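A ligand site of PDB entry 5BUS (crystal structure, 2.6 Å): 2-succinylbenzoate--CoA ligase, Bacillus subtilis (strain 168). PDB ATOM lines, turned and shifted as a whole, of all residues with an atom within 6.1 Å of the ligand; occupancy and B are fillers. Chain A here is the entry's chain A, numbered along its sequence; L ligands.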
ATOM      1  N   TYR A 153       0.877 -15.662 -31.479  1.00  0.00           N
ATOM      2  CA  TYR A 153       0.676 -15.410 -30.059  1.00  0.00           C
ATOM      3  C   TYR A 153       1.870 -14.700 -29.418  1.00  0.00           C
ATOM      4  O   TYR A 153       3.025 -14.951 -29.769  1.00  0.00           O
ATOM      5  CB  TYR A 153       0.370 -16.711 -29.322  1.00  0.00           C
ATOM      6  CG  TYR A 153      -1.076 -17.057 -29.469  1.00  0.00           C
ATOM      7  CD1 TYR A 153      -1.517 -17.791 -30.564  1.00  0.00           C
ATOM      8  CD2 TYR A 153      -2.022 -16.584 -28.551  1.00  0.00           C
ATOM      9  CE1 TYR A 153      -2.862 -18.070 -30.726  1.00  0.00           C
ATOM     10  CE2 TYR A 153      -3.359 -16.871 -28.704  1.00  0.00           C
ATOM     11  CZ  TYR A 153      -3.779 -17.604 -29.795  1.00  0.00           C
ATOM     12  OH  TYR A 153      -5.105 -17.900 -29.975  1.00  0.00           O
ATOM     13  N   THR A 154       1.576 -13.802 -28.480  1.00  0.00           N
ATOM     14  CA  THR A 154       2.619 -13.116 -27.758  1.00  0.00           C
ATOM     15  C   THR A 154       3.210 -14.115 -26.782  1.00  0.00           C
ATOM     16  O   THR A 154       2.613 -15.127 -26.500  1.00  0.00           O
ATOM     17  CB  THR A 154       2.113 -11.874 -27.001  1.00  0.00           C
ATOM     18  OG1 THR A 154       1.224 -12.295 -25.951  1.00  0.00           O
ATOM     19  CG2 THR A 154       1.424 -10.894 -27.947  1.00  0.00           C
ATOM     20  N   SER A 155       4.392 -13.812 -26.262  1.00  0.00           N
ATOM     21  CA  SER A 155       5.025 -14.683 -25.279  1.00  0.00           C
ATOM     22  C   SER A 155       5.588 -13.833 -24.142  1.00  0.00           C
ATOM     23  O   SER A 155       6.720 -14.037 -23.701  1.00  0.00           O
ATOM     24  CB  SER A 155       6.132 -15.495 -25.937  1.00  0.00           C
ATOM     25  OG  SER A 155       7.002 -14.641 -26.656  1.00  0.00           O
ATOM     26  N   HIS A 198       8.047 -17.246 -35.596  1.00  0.00           N
ATOM     27  CA  HIS A 198       8.262 -15.920 -35.028  1.00  0.00           C
ATOM     28  C   HIS A 198       8.203 -14.929 -36.191  1.00  0.00           C
ATOM     29  O   HIS A 198       8.468 -15.288 -37.352  1.00  0.00           O
ATOM     30  CB  HIS A 198       9.581 -15.814 -34.264  1.00  0.00           C
ATOM     31  CG  HIS A 198       9.810 -14.480 -33.602  1.00  0.00           C
ATOM     32  ND1 HIS A 198      10.275 -13.374 -34.283  1.00  0.00           N
ATOM     33  CD2 HIS A 198       9.663 -14.089 -32.306  1.00  0.00           C
ATOM     34  CE1 HIS A 198      10.404 -12.361 -33.450  1.00  0.00           C
ATOM     35  NE2 HIS A 198      10.024 -12.762 -32.243  1.00  0.00           N
ATOM     36  N   ILE A 199       7.847 -13.686 -35.880  1.00  0.00           N
ATOM     37  CA  ILE A 199       7.578 -12.681 -36.917  1.00  0.00           C
ATOM     38  C   ILE A 199       8.854 -12.260 -37.652  1.00  0.00           C
ATOM     39  O   ILE A 199       8.784 -11.844 -38.808  1.00  0.00           O
ATOM     40  CB  ILE A 199       6.864 -11.435 -36.292  1.00  0.00           C
ATOM     41  CG1 ILE A 199       6.267 -10.535 -37.377  1.00  0.00           C
ATOM     42  CG2 ILE A 199       7.777 -10.671 -35.270  1.00  0.00           C
ATOM     43  CD1 ILE A 199       5.381 -11.219 -38.375  1.00  0.00           C
ATOM     44  N   LEU A 264      19.601  -6.872 -36.445  1.00  0.00           N
ATOM     45  CA  LEU A 264      19.679  -7.406 -35.102  1.00  0.00           C
ATOM     46  C   LEU A 264      18.386  -7.093 -34.371  1.00  0.00           C
ATOM     47  O   LEU A 264      18.047  -5.928 -34.171  1.00  0.00           O
ATOM     48  CB  LEU A 264      20.896  -6.844 -34.364  1.00  0.00           C
ATOM     49  CG  LEU A 264      21.157  -7.372 -32.958  1.00  0.00           C
ATOM     50  CD1 LEU A 264      21.587  -8.835 -33.003  1.00  0.00           C
ATOM     51  CD2 LEU A 264      22.197  -6.502 -32.287  1.00  0.00           C
ATOM     52  N   GLY A 265      17.651  -8.138 -34.006  1.00  0.00           N
ATOM     53  CA  GLY A 265      16.447  -8.003 -33.203  1.00  0.00           C
ATOM     54  C   GLY A 265      16.607  -8.573 -31.804  1.00  0.00           C
ATOM     55  O   GLY A 265      17.602  -9.228 -31.497  1.00  0.00           O
ATOM     56  N   GLY A 266      15.620  -8.277 -30.946  1.00  0.00           N
ATOM     57  CA  GLY A 266      15.499  -8.917 -29.649  1.00  0.00           C
ATOM     58  C   GLY A 266      15.862  -8.099 -28.431  1.00  0.00           C
ATOM     59  O   GLY A 266      15.240  -8.230 -27.378  1.00  0.00           O
ATOM     60  N   GLY A 267      16.863  -7.233 -28.553  1.00  0.00           N
ATOM     61  CA  GLY A 267      17.413  -6.554 -27.397  1.00  0.00           C
ATOM     62  C   GLY A 267      18.637  -5.764 -27.806  1.00  0.00           C
ATOM     63  O   GLY A 267      19.093  -5.875 -28.937  1.00  0.00           O
ATOM     64  N   PRO A 268      19.183  -4.968 -26.874  1.00  0.00           N
ATOM     65  CA  PRO A 268      20.358  -4.149 -27.198  1.00  0.00           C
ATOM     66  C   PRO A 268      21.594  -5.016 -27.336  1.00  0.00           C
ATOM     67  O   PRO A 268      21.600  -6.173 -26.882  1.00  0.00           O
ATOM     68  CB  PRO A 268      20.490  -3.243 -25.980  1.00  0.00           C
ATOM     69  CG  PRO A 268      20.061  -4.152 -24.852  1.00  0.00           C
ATOM     70  CD  PRO A 268      18.936  -5.009 -25.422  1.00  0.00           C
ATOM     71  N   GLN A 286      20.549  -2.293 -35.557  1.00  0.00           N
ATOM     72  CA  GLN A 286      19.729  -2.598 -34.402  1.00  0.00           C
ATOM     73  C   GLN A 286      18.271  -2.196 -34.675  1.00  0.00           C
ATOM     74  O   GLN A 286      17.968  -1.327 -35.517  1.00  0.00           O
ATOM     75  CB  GLN A 286      20.307  -1.934 -33.161  1.00  0.00           C
ATOM     76  CG  GLN A 286      21.711  -2.430 -32.889  1.00  0.00           C
ATOM     77  CD  GLN A 286      22.368  -1.673 -31.776  1.00  0.00           C
ATOM     78  OE1 GLN A 286      22.182  -2.000 -30.588  1.00  0.00           O
ATOM     79  NE2 GLN A 286      23.125  -0.636 -32.132  1.00  0.00           N
ATOM     80  N   SER A 287      17.349  -2.863 -33.998  1.00  0.00           N
ATOM     81  CA  SER A 287      15.941  -2.639 -34.264  1.00  0.00           C
ATOM     82  C   SER A 287      15.087  -2.849 -33.046  1.00  0.00           C
ATOM     83  O   SER A 287      15.489  -3.474 -32.061  1.00  0.00           O
ATOM     84  CB  SER A 287      15.447  -3.564 -35.368  1.00  0.00           C
ATOM     85  OG  SER A 287      15.594  -4.909 -35.001  1.00  0.00           O
ATOM     86  N   TYR A 288      13.885  -2.292 -33.117  1.00  0.00           N
ATOM     87  CA  TYR A 288      12.879  -2.544 -32.103  1.00  0.00           C
ATOM     88  C   TYR A 288      11.616  -2.868 -32.854  1.00  0.00           C
ATOM     89  O   TYR A 288      11.346  -2.303 -33.921  1.00  0.00           O
ATOM     90  CB  TYR A 288      12.690  -1.327 -31.180  1.00  0.00           C
ATOM     91  CG  TYR A 288      11.439  -1.361 -30.348  1.00  0.00           C
ATOM     92  CD1 TYR A 288      11.366  -2.139 -29.182  1.00  0.00           C
ATOM     93  CD2 TYR A 288      10.314  -0.627 -30.714  1.00  0.00           C
ATOM     94  CE1 TYR A 288      10.217  -2.159 -28.401  1.00  0.00           C
ATOM     95  CE2 TYR A 288       9.165  -0.642 -29.950  1.00  0.00           C
ATOM     96  CZ  TYR A 288       9.114  -1.409 -28.782  1.00  0.00           C
ATOM     97  OH  TYR A 288       7.963  -1.428 -28.031  1.00  0.00           O
ATOM     98  N   GLY A 289      10.823  -3.776 -32.297  1.00  0.00           N
ATOM     99  CA  GLY A 289       9.605  -4.151 -32.976  1.00  0.00           C
ATOM    100  C   GLY A 289       9.045  -5.302 -32.213  1.00  0.00           C
ATOM    101  O   GLY A 289       9.672  -5.755 -31.267  1.00  0.00           O
ATOM    102  N   MET A 290       7.880  -5.770 -32.621  1.00  0.00           N
ATOM    103  CA  MET A 290       7.228  -6.837 -31.899  1.00  0.00           C
ATOM    104  C   MET A 290       6.267  -7.594 -32.799  1.00  0.00           C
ATOM    105  O   MET A 290       6.067  -7.223 -33.974  1.00  0.00           O
ATOM    106  CB  MET A 290       6.530  -6.284 -30.650  1.00  0.00           C
ATOM    107  CG  MET A 290       5.581  -5.133 -30.919  1.00  0.00           C
ATOM    108  SD  MET A 290       5.471  -3.919 -29.607  1.00  0.00           S
ATOM    109  CE  MET A 290       4.688  -4.861 -28.340  1.00  0.00           C
ATOM    110  N   THR A 291       5.749  -8.703 -32.262  1.00  0.00           N
ATOM    111  CA  THR A 291       4.706  -9.442 -32.951  1.00  0.00           C
ATOM    112  C   THR A 291       3.567  -8.507 -33.344  1.00  0.00           C
ATOM    113  O   THR A 291       3.126  -8.508 -34.481  1.00  0.00           O
ATOM    114  CB  THR A 291       4.170 -10.550 -32.085  1.00  0.00           C
ATOM    115  OG1 THR A 291       5.254 -11.397 -31.716  1.00  0.00           O
ATOM    116  CG2 THR A 291       3.147 -11.345 -32.848  1.00  0.00           C
ATOM    117  N   GLU A 292       3.157  -7.670 -32.405  1.00  0.00           N
ATOM    118  CA  GLU A 292       2.162  -6.641 -32.632  1.00  0.00           C
ATOM    119  C   GLU A 292       2.463  -5.688 -33.793  1.00  0.00           C
ATOM    120  O   GLU A 292       1.561  -5.072 -34.349  1.00  0.00           O
ATOM    121  CB  GLU A 292       1.983  -5.832 -31.340  1.00  0.00           C
ATOM    122  CG  GLU A 292       1.241  -6.588 -30.210  1.00  0.00           C
ATOM    123  CD  GLU A 292       2.169  -7.385 -29.307  1.00  0.00           C
ATOM    124  OE1 GLU A 292       3.265  -7.810 -29.776  1.00  0.00           O
ATOM    125  OE2 GLU A 292       1.773  -7.618 -28.130  1.00  0.00           O
ATOM    126  N   ALA A 312      17.585   2.048 -30.074  1.00  0.00           N
ATOM    127  CA  ALA A 312      17.008   1.173 -31.090  1.00  0.00           C
ATOM    128  C   ALA A 312      16.856   1.928 -32.407  1.00  0.00           C
ATOM    129  O   ALA A 312      16.532   1.330 -33.431  1.00  0.00           O
ATOM    130  CB  ALA A 312      15.655   0.619 -30.641  1.00  0.00           C
ATOM    131  N   THR A 367       2.646  -0.372 -26.118  1.00  0.00           N
ATOM    132  CA  THR A 367       3.462  -1.576 -26.281  1.00  0.00           C
ATOM    133  C   THR A 367       3.722  -2.371 -25.020  1.00  0.00           C
ATOM    134  O   THR A 367       4.119  -3.539 -25.098  1.00  0.00           O
ATOM    135  CB  THR A 367       4.851  -1.246 -26.870  1.00  0.00           C
ATOM    136  OG1 THR A 367       5.561  -0.389 -25.965  1.00  0.00           O
ATOM    137  CG2 THR A 367       4.739  -0.607 -28.251  1.00  0.00           C
ATOM    138  N   ASP A 369       6.079  -1.496 -23.180  1.00  0.00           N
ATOM    139  CA  ASP A 369       7.515  -1.266 -23.003  1.00  0.00           C
ATOM    140  C   ASP A 369       7.768   0.106 -22.416  1.00  0.00           C
ATOM    141  O   ASP A 369       7.142   1.085 -22.809  1.00  0.00           O
ATOM    142  CB  ASP A 369       8.266  -1.400 -24.347  1.00  0.00           C
ATOM    143  CG  ASP A 369       8.351  -2.840 -24.831  1.00  0.00           C
ATOM    144  OD1 ASP A 369       8.554  -3.724 -23.976  1.00  0.00           O
ATOM    145  OD2 ASP A 369       8.241  -3.065 -26.054  1.00  0.00           O
ATOM    146  N   VAL A 381      15.131   1.739 -25.288  1.00  0.00           N
ATOM    147  CA  VAL A 381      14.187   0.831 -24.673  1.00  0.00           C
ATOM    148  C   VAL A 381      14.652   0.345 -23.321  1.00  0.00           C
ATOM    149  O   VAL A 381      15.661  -0.292 -23.215  1.00  0.00           O
ATOM    150  CB  VAL A 381      13.980  -0.391 -25.573  1.00  0.00           C
ATOM    151  CG1 VAL A 381      12.780  -1.181 -25.129  1.00  0.00           C
ATOM    152  CG2 VAL A 381      13.805   0.032 -27.006  1.00  0.00           C
ATOM    153  N   ASP A 383      12.731  -1.747 -20.962  1.00  0.00           N
ATOM    154  CA  ASP A 383      12.194  -3.088 -20.721  1.00  0.00           C
ATOM    155  C   ASP A 383      10.781  -2.992 -20.215  1.00  0.00           C
ATOM    156  O   ASP A 383      10.205  -1.947 -20.268  1.00  0.00           O
ATOM    157  CB  ASP A 383      13.078  -4.075 -19.917  1.00  0.00           C
ATOM    158  CG  ASP A 383      13.065  -3.841 -18.448  1.00  0.00           C
ATOM    159  OD1 ASP A 383      13.828  -4.508 -17.735  1.00  0.00           O
ATOM    160  OD2 ASP A 383      12.306  -2.995 -17.988  1.00  0.00           O
ATOM    161  N   ARG A 384      10.220  -4.099 -19.771  1.00  0.00           N
ATOM    162  CA  ARG A 384       8.792  -4.145 -19.576  1.00  0.00           C
ATOM    163  C   ARG A 384       8.276  -3.422 -18.375  1.00  0.00           C
ATOM    164  O   ARG A 384       8.779  -3.553 -17.290  1.00  0.00           O
ATOM    165  CB  ARG A 384       8.290  -5.576 -19.577  1.00  0.00           C
ATOM    166  CG  ARG A 384       8.725  -6.413 -20.742  1.00  0.00           C
ATOM    167  CD  ARG A 384       7.970  -6.079 -21.996  1.00  0.00           C
ATOM    168  NE  ARG A 384       6.552  -6.301 -21.857  1.00  0.00           N
ATOM    169  CZ  ARG A 384       5.674  -5.968 -22.765  1.00  0.00           C
ATOM    170  NH1 ARG A 384       4.408  -6.196 -22.570  1.00  0.00           N
ATOM    171  NH2 ARG A 384       6.063  -5.403 -23.854  1.00  0.00           N
ATOM    172  N   SER A 471       9.820 -18.942 -25.586  1.00  0.00           N
ATOM    173  CA  SER A 471      10.546 -18.017 -26.456  1.00  0.00           C
ATOM    174  C   SER A 471      11.868 -17.582 -25.842  1.00  0.00           C
ATOM    175  O   SER A 471      12.423 -16.553 -26.238  1.00  0.00           O
ATOM    176  CB  SER A 471       9.683 -16.785 -26.759  1.00  0.00           C
ATOM    177  OG  SER A 471       8.596 -17.148 -27.588  1.00  0.00           O
ATOM    178  N   LYS A 473      12.434 -16.336 -23.126  1.00  0.00           N
ATOM    179  CA  LYS A 473      12.250 -15.145 -22.314  1.00  0.00           C
ATOM    180  C   LYS A 473      12.195 -15.437 -20.814  1.00  0.00           C
ATOM    181  O   LYS A 473      11.467 -16.317 -20.361  1.00  0.00           O
ATOM    182  CB  LYS A 473      10.985 -14.401 -22.753  1.00  0.00           C
ATOM    183  CG  LYS A 473      11.137 -13.658 -24.086  1.00  0.00           C
ATOM    184  CD  LYS A 473       9.835 -13.009 -24.498  1.00  0.00           C
ATOM    185  CE  LYS A 473       9.901 -12.448 -25.914  1.00  0.00           C
ATOM    186  NZ  LYS A 473       8.521 -12.201 -26.466  1.00  0.00           N
HETATM  187  P1  LIG L   1       8.163 -10.628 -29.556  1.00  0.00           P
HETATM  188  O1  LIG L   1       6.785 -10.291 -29.861  1.00  0.00           O
HETATM  189  O2  LIG L   1       9.085 -10.378 -30.644  1.00  0.00           O
HETATM  190  O3  LIG L   1       8.356 -11.901 -28.896  1.00  0.00           O
HETATM  191  O4  LIG L   1       8.569  -9.640 -28.427  1.00  0.00           O
HETATM  192  C1  LIG L   1       8.730  -8.241 -28.608  1.00  0.00           C
HETATM  193  C2  LIG L   1       9.292  -7.634 -27.348  1.00  0.00           C
HETATM  194  O5  LIG L   1      10.685  -7.819 -27.317  1.00  0.00           O
HETATM  195  C3  LIG L   1       9.171  -6.127 -27.277  1.00  0.00           C
HETATM  196  O6  LIG L   1       8.012  -5.731 -26.607  1.00  0.00           O
HETATM  197  C4  LIG L   1      10.299  -5.718 -26.400  1.00  0.00           C
HETATM  198  O7  LIG L   1       9.864  -5.787 -25.079  1.00  0.00           O
HETATM  199  C5  LIG L   1      11.335  -6.756 -26.658  1.00  0.00           C
HETATM  200  N1  LIG L   1      12.270  -6.132 -27.599  1.00  0.00           N
HETATM  201  C6  LIG L   1      12.271  -6.280 -28.901  1.00  0.00           C
HETATM  202  N2  LIG L   1      13.236  -5.577 -29.497  1.00  0.00           N
HETATM  203  C7  LIG L   1      13.883  -4.935 -28.547  1.00  0.00           C
HETATM  204  C8  LIG L   1      15.016  -4.019 -28.444  1.00  0.00           C
HETATM  205  N3  LIG L   1      15.708  -3.594 -29.493  1.00  0.00           N
HETATM  206  N4  LIG L   1      15.367  -3.590 -27.257  1.00  0.00           N
HETATM  207  C9  LIG L   1      14.723  -3.971 -26.167  1.00  0.00           C
HETATM  208  N5  LIG L   1      13.700  -4.795 -26.175  1.00  0.00           N
HETATM  209  C10 LIG L   1      13.244  -5.309 -27.303  1.00  0.00           C
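The side-chain hydroxyl (OH) of Tyr 288 lies close to the side-chain hydroxyl (OG1) of Thr 367 (3.3 Å). The backbone NH (N) of Asp 369 sits at hydrogen-bond distance from the side-chain hydroxyl (OG1) of Thr 367. OD2 of Asp 369 lies within hydrogen-bond range of OH of Tyr 288 (2.6 Å). The side-chain hydroxyl (OG) of Ser 155 lies within hydrogen-bond range of the side-chain amino group (NZ) of Lys 473 (2.9 Å). The side-chain hydroxyl of Ser 155 is in hydrogen-bond range of the side-chain hydroxyl of Ser 471 (3.1 Å). The guanidinium group of Arg 384 sits at hydrogen-bond distance from the backbone carbonyl oxygen of Thr 367, 3.0 Å away. OG of Ser 287 is in hydrogen-bond range of O of Leu 264, at 2.8 Å. The side-chain carboxylate (OD1) of Asp 369 is in salt-bridge range of the guanidinium group (NH2) of Arg 384, at 3.0 Å.
Ser 155 touches the ligand (OG to O3, 3.8 Å). O of Gly 266 touches C10 of the ligand, 3.5 Å away. Gly 267 touches the ligand. Tyr 288 touches the ligand (CD1 to C7, 3.8 Å). Gly 289 touches the ligand. Met 290 touches the ligand (CB to C1, 3.6 Å). Val 381 touches the ligand (CG1 to C9, 3.6 Å). Of the 25 residues printed, 13 come within 4 Å of the ligand. The nearest printed residue that does not touch the ligand is Pro 268 (4.1 Å).
An oxygen (O2) of the ligand is in hydrogen-bond range of a ring nitrogen (NE2) of His 198, 3.0 Å away. The backbone NH (N) of Thr 291 sits at hydrogen-bond distance from an oxygen (O1) of the ligand. NZ of Lys 473 is in salt-bridge range of O3 of the ligand (2.5 Å). An oxygen (O7) of the ligand is in hydrogen-bond range of the side-chain carboxylate (OD1) of Asp 369. A nitrogen (N3) of the ligand is in hydrogen-bond range of the backbone carbonyl oxygen (O) of Ser 287 (2.6 Å). An oxygen (O1) of the ligand is in hydrogen-bond range of the side-chain hydroxyl of Thr 291 (2.6 Å). NH2 of Arg 384 sits at hydrogen-bond distance from O6 of the ligand, 3.4 Å away.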
